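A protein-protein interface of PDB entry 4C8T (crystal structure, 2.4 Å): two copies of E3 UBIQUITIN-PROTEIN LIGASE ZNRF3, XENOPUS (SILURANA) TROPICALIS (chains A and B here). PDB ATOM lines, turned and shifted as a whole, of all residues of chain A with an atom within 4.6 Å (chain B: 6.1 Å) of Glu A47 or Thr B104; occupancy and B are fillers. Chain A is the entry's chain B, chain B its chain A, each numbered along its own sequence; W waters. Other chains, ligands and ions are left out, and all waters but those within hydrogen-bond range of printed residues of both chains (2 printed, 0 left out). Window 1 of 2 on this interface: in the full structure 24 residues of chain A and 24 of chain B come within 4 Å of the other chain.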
ATOM      1  N   ALA A  46      15.900 -20.113 -18.300  1.00  0.00           N
ATOM      2  CA  ALA A  46      15.465 -19.829 -19.671  1.00  0.00           C
ATOM      3  C   ALA A  46      15.559 -18.340 -19.965  1.00  0.00           C
ATOM      4  O   ALA A  46      15.665 -17.527 -19.040  1.00  0.00           O
ATOM      5  CB  ALA A  46      14.037 -20.314 -19.883  1.00  0.00           C
ATOM      6  N   GLU A  47      15.498 -17.988 -21.248  1.00  0.00           N
ATOM      7  CA  GLU A  47      15.782 -16.616 -21.693  1.00  0.00           C
ATOM      8  C   GLU A  47      15.273 -16.335 -23.131  1.00  0.00           C
ATOM      9  O   GLU A  47      15.211 -17.239 -23.980  1.00  0.00           O
ATOM     10  CB  GLU A  47      17.296 -16.345 -21.605  1.00  0.00           C
ATOM     11  CG  GLU A  47      17.792 -15.085 -22.330  1.00  0.00           C
ATOM     12  CD  GLU A  47      19.291 -14.970 -22.395  1.00  0.00           C
ATOM     13  OE1 GLU A  47      19.990 -15.972 -22.280  1.00  0.00           O
ATOM     14  OE2 GLU A  47      19.801 -13.859 -22.539  1.00  0.00           O
ATOM     15  N   GLY A  48      14.945 -15.063 -23.377  1.00  0.00           N
ATOM     16  CA  GLY A  48      14.396 -14.605 -24.635  1.00  0.00           C
ATOM     17  C   GLY A  48      13.608 -13.306 -24.457  1.00  0.00           C
ATOM     18  O   GLY A  48      13.398 -12.790 -23.351  1.00  0.00           O
ATOM     19  N   GLY A  71      11.099 -18.773 -29.057  1.00  0.00           N
ATOM     20  CA  GLY A  71      11.933 -18.546 -27.868  1.00  0.00           C
ATOM     21  C   GLY A  71      11.612 -17.267 -27.147  1.00  0.00           C
ATOM     22  O   GLY A  71      12.465 -16.687 -26.538  1.00  0.00           O
ATOM     23  N   VAL A  73       9.667 -15.037 -24.101  1.00  0.00           N
ATOM     24  CA  VAL A  73       9.243 -15.154 -22.742  1.00  0.00           C
ATOM     25  C   VAL A  73       7.899 -14.474 -22.605  1.00  0.00           C
ATOM     26  O   VAL A  73       7.815 -13.257 -22.572  1.00  0.00           O
ATOM     27  CB  VAL A  73      10.300 -14.603 -21.765  1.00  0.00           C
ATOM     28  CG1 VAL A  73       9.720 -14.412 -20.371  1.00  0.00           C
ATOM     29  CG2 VAL A  73      11.460 -15.590 -21.691  1.00  0.00           C
ATOM     30  N   THR A 104       9.585 -19.910 -24.811  1.00  0.00           N
ATOM     31  CA  THR A 104      10.599 -20.632 -24.029  1.00  0.00           C
ATOM     32  C   THR A 104      10.328 -20.613 -22.523  1.00  0.00           C
ATOM     33  O   THR A 104      10.975 -21.302 -21.751  1.00  0.00           O
ATOM     34  CB  THR A 104      12.032 -20.050 -24.268  1.00  0.00           C
ATOM     35  OG1 THR A 104      13.006 -20.830 -23.568  1.00  0.00           O
ATOM     36  CG2 THR A 104      12.175 -18.597 -23.831  1.00  0.00           C
ATOM     37  N   ARG A 154      14.489  -7.965 -22.552  1.00  0.00           N
ATOM     38  CA  ARG A 154      14.863  -9.368 -22.521  1.00  0.00           C
ATOM     39  C   ARG A 154      14.722  -9.945 -21.094  1.00  0.00           C
ATOM     40  O   ARG A 154      15.010  -9.265 -20.118  1.00  0.00           O
ATOM     41  CB  ARG A 154      16.286  -9.548 -23.073  1.00  0.00           C
ATOM     42  CG  ARG A 154      16.574 -10.987 -23.473  1.00  0.00           C
ATOM     43  CD  ARG A 154      17.809 -11.159 -24.305  1.00  0.00           C
ATOM     44  NE  ARG A 154      17.981 -12.539 -24.749  1.00  0.00           N
ATOM     45  CZ  ARG A 154      17.566 -13.031 -25.910  1.00  0.00           C
ATOM     46  NH1 ARG A 154      16.935 -12.257 -26.784  1.00  0.00           N
ATOM     47  NH2 ARG A 154      17.809 -14.316 -26.205  1.00  0.00           N
ATOM     48  N   ALA A 155      14.250 -11.189 -20.972  1.00  0.00           N
ATOM     49  CA  ALA A 155      14.137 -11.831 -19.652  1.00  0.00           C
ATOM     50  C   ALA A 155      15.163 -12.941 -19.546  1.00  0.00           C
ATOM     51  O   ALA A 155      15.315 -13.732 -20.482  1.00  0.00           O
ATOM     52  CB  ALA A 155      12.753 -12.376 -19.456  1.00  0.00           C
ATOM     53  N   ARG A 156      15.920 -12.955 -18.457  1.00  0.00           N
ATOM     54  CA  ARG A 156      16.820 -14.079 -18.190  1.00  0.00           C
ATOM     55  C   ARG A 156      16.333 -14.698 -16.913  1.00  0.00           C
ATOM     56  O   ARG A 156      16.431 -14.074 -15.849  1.00  0.00           O
ATOM     57  CB  ARG A 156      18.261 -13.605 -18.062  1.00  0.00           C
ATOM     58  CG  ARG A 156      18.848 -13.165 -19.381  1.00  0.00           C
ATOM     59  CD  ARG A 156      20.130 -12.379 -19.260  1.00  0.00           C
ATOM     60  NE  ARG A 156      20.749 -12.270 -20.574  1.00  0.00           N
ATOM     61  CZ  ARG A 156      21.557 -11.285 -20.968  1.00  0.00           C
ATOM     62  NH1 ARG A 156      21.881 -10.273 -20.160  1.00  0.00           N
ATOM     63  NH2 ARG A 156      22.037 -11.315 -22.210  1.00  0.00           N
ATOM     64  N   SER B  45      23.528 -19.901 -17.184  1.00  0.00           N
ATOM     65  CA  SER B  45      22.730 -20.254 -18.325  1.00  0.00           C
ATOM     66  C   SER B  45      22.462 -19.025 -19.209  1.00  0.00           C
ATOM     67  O   SER B  45      22.443 -17.848 -18.750  1.00  0.00           O
ATOM     68  CB  SER B  45      21.419 -20.875 -17.885  1.00  0.00           C
ATOM     69  OG  SER B  45      21.574 -22.264 -17.659  1.00  0.00           O
ATOM     70  N   ALA B  46      22.258 -19.332 -20.483  1.00  0.00           N
ATOM     71  CA  ALA B  46      22.043 -18.355 -21.515  1.00  0.00           C
ATOM     72  C   ALA B  46      21.354 -19.029 -22.704  1.00  0.00           C
ATOM     73  O   ALA B  46      21.563 -20.225 -22.997  1.00  0.00           O
ATOM     74  CB  ALA B  46      23.366 -17.739 -21.952  1.00  0.00           C
ATOM     75  N   GLU B  47      20.526 -18.243 -23.375  1.00  0.00           N
ATOM     76  CA  GLU B  47      19.725 -18.727 -24.448  1.00  0.00           C
ATOM     77  C   GLU B  47      19.452 -17.594 -25.469  1.00  0.00           C
ATOM     78  O   GLU B  47      19.242 -16.408 -25.121  1.00  0.00           O
ATOM     79  CB  GLU B  47      18.421 -19.327 -23.915  1.00  0.00           C
ATOM     80  CG  GLU B  47      17.305 -19.412 -24.966  1.00  0.00           C
ATOM     81  CD  GLU B  47      15.972 -19.872 -24.426  1.00  0.00           C
ATOM     82  OE1 GLU B  47      15.819 -20.036 -23.198  1.00  0.00           O
ATOM     83  OE2 GLU B  47      15.059 -20.057 -25.245  1.00  0.00           O
ATOM     84  N   GLY B  48      19.434 -17.992 -26.728  1.00  0.00           N
ATOM     85  CA  GLY B  48      19.189 -17.065 -27.785  1.00  0.00           C
ATOM     86  C   GLY B  48      19.529 -17.653 -29.128  1.00  0.00           C
ATOM     87  O   GLY B  48      20.035 -18.780 -29.251  1.00  0.00           O
ATOM     88  N   TYR B  70      19.838  -7.663 -30.097  1.00  0.00           N
ATOM     89  CA  TYR B  70      20.349  -8.010 -28.770  1.00  0.00           C
ATOM     90  C   TYR B  70      19.963  -9.455 -28.362  1.00  0.00           C
ATOM     91  O   TYR B  70      18.835  -9.885 -28.581  1.00  0.00           O
ATOM     92  CB  TYR B  70      19.857  -6.996 -27.722  1.00  0.00           C
ATOM     93  CG  TYR B  70      20.478  -7.198 -26.377  1.00  0.00           C
ATOM     94  CD1 TYR B  70      21.752  -6.705 -26.088  1.00  0.00           C
ATOM     95  CD2 TYR B  70      19.809  -7.905 -25.383  1.00  0.00           C
ATOM     96  CE1 TYR B  70      22.331  -6.918 -24.838  1.00  0.00           C
ATOM     97  CE2 TYR B  70      20.384  -8.121 -24.129  1.00  0.00           C
ATOM     98  CZ  TYR B  70      21.639  -7.641 -23.867  1.00  0.00           C
ATOM     99  OH  TYR B  70      22.196  -7.867 -22.639  1.00  0.00           O
ATOM    100  N   GLY B  71      20.918 -10.204 -27.803  1.00  0.00           N
ATOM    101  CA  GLY B  71      20.623 -11.473 -27.114  1.00  0.00           C
ATOM    102  C   GLY B  71      20.970 -12.749 -27.858  1.00  0.00           C
ATOM    103  O   GLY B  71      20.520 -13.838 -27.506  1.00  0.00           O
ATOM    104  N   TRP B  72      21.800 -12.608 -28.859  1.00  0.00           N
ATOM    105  CA  TRP B  72      22.148 -13.716 -29.740  1.00  0.00           C
ATOM    106  C   TRP B  72      23.282 -14.528 -29.088  1.00  0.00           C
ATOM    107  O   TRP B  72      24.006 -14.033 -28.262  1.00  0.00           O
ATOM    108  CB  TRP B  72      22.610 -13.207 -31.134  1.00  0.00           C
ATOM    109  CG  TRP B  72      23.563 -12.079 -31.111  1.00  0.00           C
ATOM    110  CD1 TRP B  72      23.265 -10.796 -30.822  1.00  0.00           C
ATOM    111  CD2 TRP B  72      24.970 -12.103 -31.409  1.00  0.00           C
ATOM    112  NE1 TRP B  72      24.419 -10.001 -30.873  1.00  0.00           N
ATOM    113  CE2 TRP B  72      25.469 -10.800 -31.235  1.00  0.00           C
ATOM    114  CE3 TRP B  72      25.858 -13.101 -31.784  1.00  0.00           C
ATOM    115  CZ2 TRP B  72      26.809 -10.468 -31.455  1.00  0.00           C
ATOM    116  CZ3 TRP B  72      27.205 -12.775 -31.981  1.00  0.00           C
ATOM    117  CH2 TRP B  72      27.664 -11.470 -31.832  1.00  0.00           C
ATOM    118  N   VAL B  73      23.422 -15.765 -29.518  1.00  0.00           N
ATOM    119  CA  VAL B  73      24.407 -16.656 -29.026  1.00  0.00           C
ATOM    120  C   VAL B  73      25.297 -16.882 -30.192  1.00  0.00           C
ATOM    121  O   VAL B  73      24.920 -17.557 -31.113  1.00  0.00           O
ATOM    122  CB  VAL B  73      23.798 -17.980 -28.488  1.00  0.00           C
ATOM    123  CG1 VAL B  73      24.847 -19.083 -28.398  1.00  0.00           C
ATOM    124  CG2 VAL B  73      23.197 -17.720 -27.109  1.00  0.00           C
ATOM    125  N   GLY B  74      26.476 -16.270 -30.136  1.00  0.00           N
ATOM    126  CA  GLY B  74      27.446 -16.337 -31.209  1.00  0.00           C
ATOM    127  C   GLY B  74      28.187 -17.658 -31.211  1.00  0.00           C
ATOM    128  O   GLY B  74      28.512 -18.219 -30.150  1.00  0.00           O
ATOM    129  N   ALA B  98      31.958  -9.437 -28.887  1.00  0.00           N
ATOM    130  CA  ALA B  98      30.651 -10.035 -29.182  1.00  0.00           C
ATOM    131  C   ALA B  98      29.553  -9.698 -28.154  1.00  0.00           C
ATOM    132  O   ALA B  98      28.400  -9.421 -28.520  1.00  0.00           O
ATOM    133  CB  ALA B  98      30.793 -11.555 -29.303  1.00  0.00           C
ATOM    134  N   VAL B  99      29.900  -9.740 -26.873  1.00  0.00           N
ATOM    135  CA  VAL B  99      28.956  -9.347 -25.827  1.00  0.00           C
ATOM    136  C   VAL B  99      28.527  -7.884 -26.015  1.00  0.00           C
ATOM    137  O   VAL B  99      27.342  -7.571 -26.053  1.00  0.00           O
ATOM    138  CB  VAL B  99      29.552  -9.561 -24.410  1.00  0.00           C
ATOM    139  CG1 VAL B  99      28.692  -8.867 -23.368  1.00  0.00           C
ATOM    140  CG2 VAL B  99      29.695 -11.054 -24.109  1.00  0.00           C
ATOM    141  N   GLY B 102      25.907  -7.109 -28.255  1.00  0.00           N
ATOM    142  CA  GLY B 102      24.674  -7.779 -27.881  1.00  0.00           C
ATOM    143  C   GLY B 102      24.646  -9.299 -27.848  1.00  0.00           C
ATOM    144  O   GLY B 102      23.569  -9.863 -27.757  1.00  0.00           O
ATOM    145  N   ALA B 103      25.780  -9.991 -27.895  1.00  0.00           N
ATOM    146  CA  ALA B 103      25.764 -11.465 -27.627  1.00  0.00           C
ATOM    147  C   ALA B 103      25.372 -11.764 -26.175  1.00  0.00           C
ATOM    148  O   ALA B 103      25.786 -11.065 -25.299  1.00  0.00           O
ATOM    149  CB  ALA B 103      27.114 -12.104 -27.924  1.00  0.00           C
ATOM    150  N   THR B 104      24.545 -12.778 -25.951  1.00  0.00           N
ATOM    151  CA  THR B 104      24.235 -13.274 -24.605  1.00  0.00           C
ATOM    152  C   THR B 104      25.241 -14.332 -24.152  1.00  0.00           C
ATOM    153  O   THR B 104      25.380 -14.597 -22.985  1.00  0.00           O
ATOM    154  CB  THR B 104      22.813 -13.888 -24.532  1.00  0.00           C
ATOM    155  OG1 THR B 104      22.404 -14.000 -23.173  1.00  0.00           O
ATOM    156  CG2 THR B 104      22.743 -15.274 -25.162  1.00  0.00           C
ATOM    157  N   ALA B 105      25.926 -14.958 -25.099  1.00  0.00           N
ATOM    158  CA  ALA B 105      26.935 -15.969 -24.796  1.00  0.00           C
ATOM    159  C   ALA B 105      27.765 -16.152 -26.052  1.00  0.00           C
ATOM    160  O   ALA B 105      27.306 -15.792 -27.153  1.00  0.00           O
ATOM    161  CB  ALA B 105      26.276 -17.285 -24.461  1.00  0.00           C
ATOM    162  N   VAL B 106      28.957 -16.732 -25.902  1.00  0.00           N
ATOM    163  CA  VAL B 106      29.777 -17.102 -27.059  1.00  0.00           C
ATOM    164  C   VAL B 106      30.071 -18.597 -26.948  1.00  0.00           C
ATOM    165  O   VAL B 106      30.301 -19.089 -25.852  1.00  0.00           O
ATOM    166  CB  VAL B 106      31.052 -16.262 -27.132  1.00  0.00           C
ATOM    167  CG1 VAL B 106      31.869 -16.601 -28.357  1.00  0.00           C
ATOM    168  CG2 VAL B 106      30.711 -14.792 -27.166  1.00  0.00           C
ATOM    169  N   ARG B 130      28.769 -12.997 -18.908  1.00  0.00           N
ATOM    170  CA  ARG B 130      28.103 -13.918 -19.830  1.00  0.00           C
ATOM    171  C   ARG B 130      28.937 -15.173 -20.016  1.00  0.00           C
ATOM    172  O   ARG B 130      30.135 -15.153 -19.800  1.00  0.00           O
ATOM    173  CB  ARG B 130      27.875 -13.239 -21.189  1.00  0.00           C
ATOM    174  CG  ARG B 130      27.141 -11.901 -21.118  1.00  0.00           C
ATOM    175  CD  ARG B 130      25.894 -11.982 -20.265  1.00  0.00           C
ATOM    176  NE  ARG B 130      24.990 -13.051 -20.692  1.00  0.00           N
ATOM    177  CZ  ARG B 130      24.083 -13.668 -19.925  1.00  0.00           C
ATOM    178  NH1 ARG B 130      23.913 -13.359 -18.650  1.00  0.00           N
ATOM    179  NH2 ARG B 130      23.333 -14.633 -20.442  1.00  0.00           N
ATOM    180  N   PRO B 131      28.299 -16.281 -20.404  1.00  0.00           N
ATOM    181  CA  PRO B 131      29.083 -17.489 -20.576  1.00  0.00           C
ATOM    182  C   PRO B 131      29.864 -17.505 -21.849  1.00  0.00           C
ATOM    183  O   PRO B 131      29.350 -17.109 -22.899  1.00  0.00           O
ATOM    184  CB  PRO B 131      28.024 -18.612 -20.636  1.00  0.00           C
ATOM    185  CG  PRO B 131      26.724 -17.938 -20.865  1.00  0.00           C
ATOM    186  CD  PRO B 131      26.849 -16.540 -20.358  1.00  0.00           C
ATOM    187  N   ARG B 154      17.991 -22.100 -32.307  1.00  0.00           N
ATOM    188  CA  ARG B 154      18.092 -21.479 -31.000  1.00  0.00           C
ATOM    189  C   ARG B 154      19.044 -22.289 -30.132  1.00  0.00           C
ATOM    190  O   ARG B 154      19.009 -23.509 -30.185  1.00  0.00           O
ATOM    191  CB  ARG B 154      16.712 -21.366 -30.336  1.00  0.00           C
ATOM    192  CG  ARG B 154      16.731 -20.487 -29.101  1.00  0.00           C
ATOM    193  CD  ARG B 154      15.407 -19.814 -28.859  1.00  0.00           C
ATOM    194  NE  ARG B 154      15.408 -18.872 -27.737  1.00  0.00           N
ATOM    195  CZ  ARG B 154      15.543 -17.554 -27.832  1.00  0.00           C
ATOM    196  NH1 ARG B 154      15.709 -16.958 -29.006  1.00  0.00           N
ATOM    197  NH2 ARG B 154      15.508 -16.801 -26.734  1.00  0.00           N
HETATM  198  O   HOH W   1      14.125 -14.204 -27.922  1.00  0.00           O
HETATM  199  O   HOH W   2      17.473 -14.521 -29.247  1.00  0.00           O
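Of the 9 printed residues of chain A, 7 touch a printed residue of chain B.
Hydrophobic or aromatic side chains of chain A that line the printed part of chain B: Ala A46.
Water W2 lies within hydrogen-bond range of NH1 of Arg B154 (3.0 Å) and NH2 of Arg A154 (3.1 Å).
Water W1 bridges NH2 of Arg B154 (3.2 Å) and O of Gly A71 (3.3 Å).
OE2 of Glu B47 is in hydrogen-bond range of OG1 of Thr A104 (2.8 Å).
NH2 of Arg B154 is in hydrogen-bond range of O of Gly A71 (3.1 Å).
The guanidinium group (NH2) of Arg A154 lies close to the guanidinium group (NH2) of Arg B154, 3.4 Å away.
O of Gly B71 is in hydrogen-bond range of NH2 of Arg A154 (3.0 Å).
NH2 of Arg A154 is in hydrogen-bond range of O of Glu B47.
The side-chain hydroxyl of Tyr B70 is in hydrogen-bond range of the guanidinium group of Arg A156 (3.5 Å).
The guanidinium group (NH2) of Arg A156 lies within hydrogen-bond range of the side-chain hydroxyl (OG1) of Thr B104 (2.9 Å).
The guanidinium group (NH2) of Arg B154 sits at hydrogen-bond distance from the backbone carbonyl oxygen (O) of Glu A47 (2.8 Å).
The side-chain hydroxyl (OG1) of Thr B104 is in hydrogen-bond range of the side-chain carboxylate (OE2) of Glu A47.
OE1 of Glu A47 is in hydrogen-bond range of N of Glu B47, 2.6 Å away.
Of chain B, only Ala B46, Glu B47, Thr B104 and Arg B154 come within 4 Å of Glu A47.
Printed residues of chain B within 4 Å of Gly A71: Arg B154.
Of the printed residues of chain B, Thr A104 touches Glu B47.
Printed residues of chain A within 4 Å of Glu B47: Ala A46, Glu A47, Thr A104 and Arg A154.
The nearest residue of chain B that does not touch Glu A47 is Arg B130 (4.04 Å).
Ala A46 touches Glu B47.
OE1 of Glu A47 touches CA of Ala B46, 3.2 Å away.
CA of Gly A48 touches NH2 of Arg B154, 3.2 Å away.
CA of Gly B48 touches NH2 of Arg A154, at 3.5 Å.
O of Tyr B70 touches NH1 of Arg A154 (3.5 Å).
NH2 of Arg B130 touches NE of Arg A156 (3.5 Å).
The guanidinium group of Arg B130 lies within hydrogen-bond range of the backbone carbonyl oxygen of Thr B104, 2.8 Å away.
The backbone carbonyl oxygen of Trp B72 sits at hydrogen-bond distance from the backbone NH of Thr B104 (2.7 Å).
O of Gly B102 lies within hydrogen-bond range of N of Gly B71 (2.7 Å).
OE2 of Glu A47 is in salt-bridge range of NE of Arg A156, 2.7 Å away.
The side-chain carboxylate (OE2) of Glu B47 lies within salt-bridge range of the guanidinium group (NE) of Arg B154 (2.8 Å).
O of Gly A48 lies within hydrogen-bond range of N of Ala A155, 3.0 Å away.
Ala A46 touches Glu B47, and with the chains exchanged Glu A47 touches Ala B46.
Glu A47 touches Thr B104, and with the chains exchanged Thr A104 touches Glu B47.
Gly A48 touches Arg B154, and with the chains exchanged Arg A154 touches Gly B48.
Arg A154 touches its own counterpart, Arg B154.
7 positions are printed for both chains.
Of the 16 pairs that touch across the chains among the printed residues, 12 have their exchanged pair printed and touching as well.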
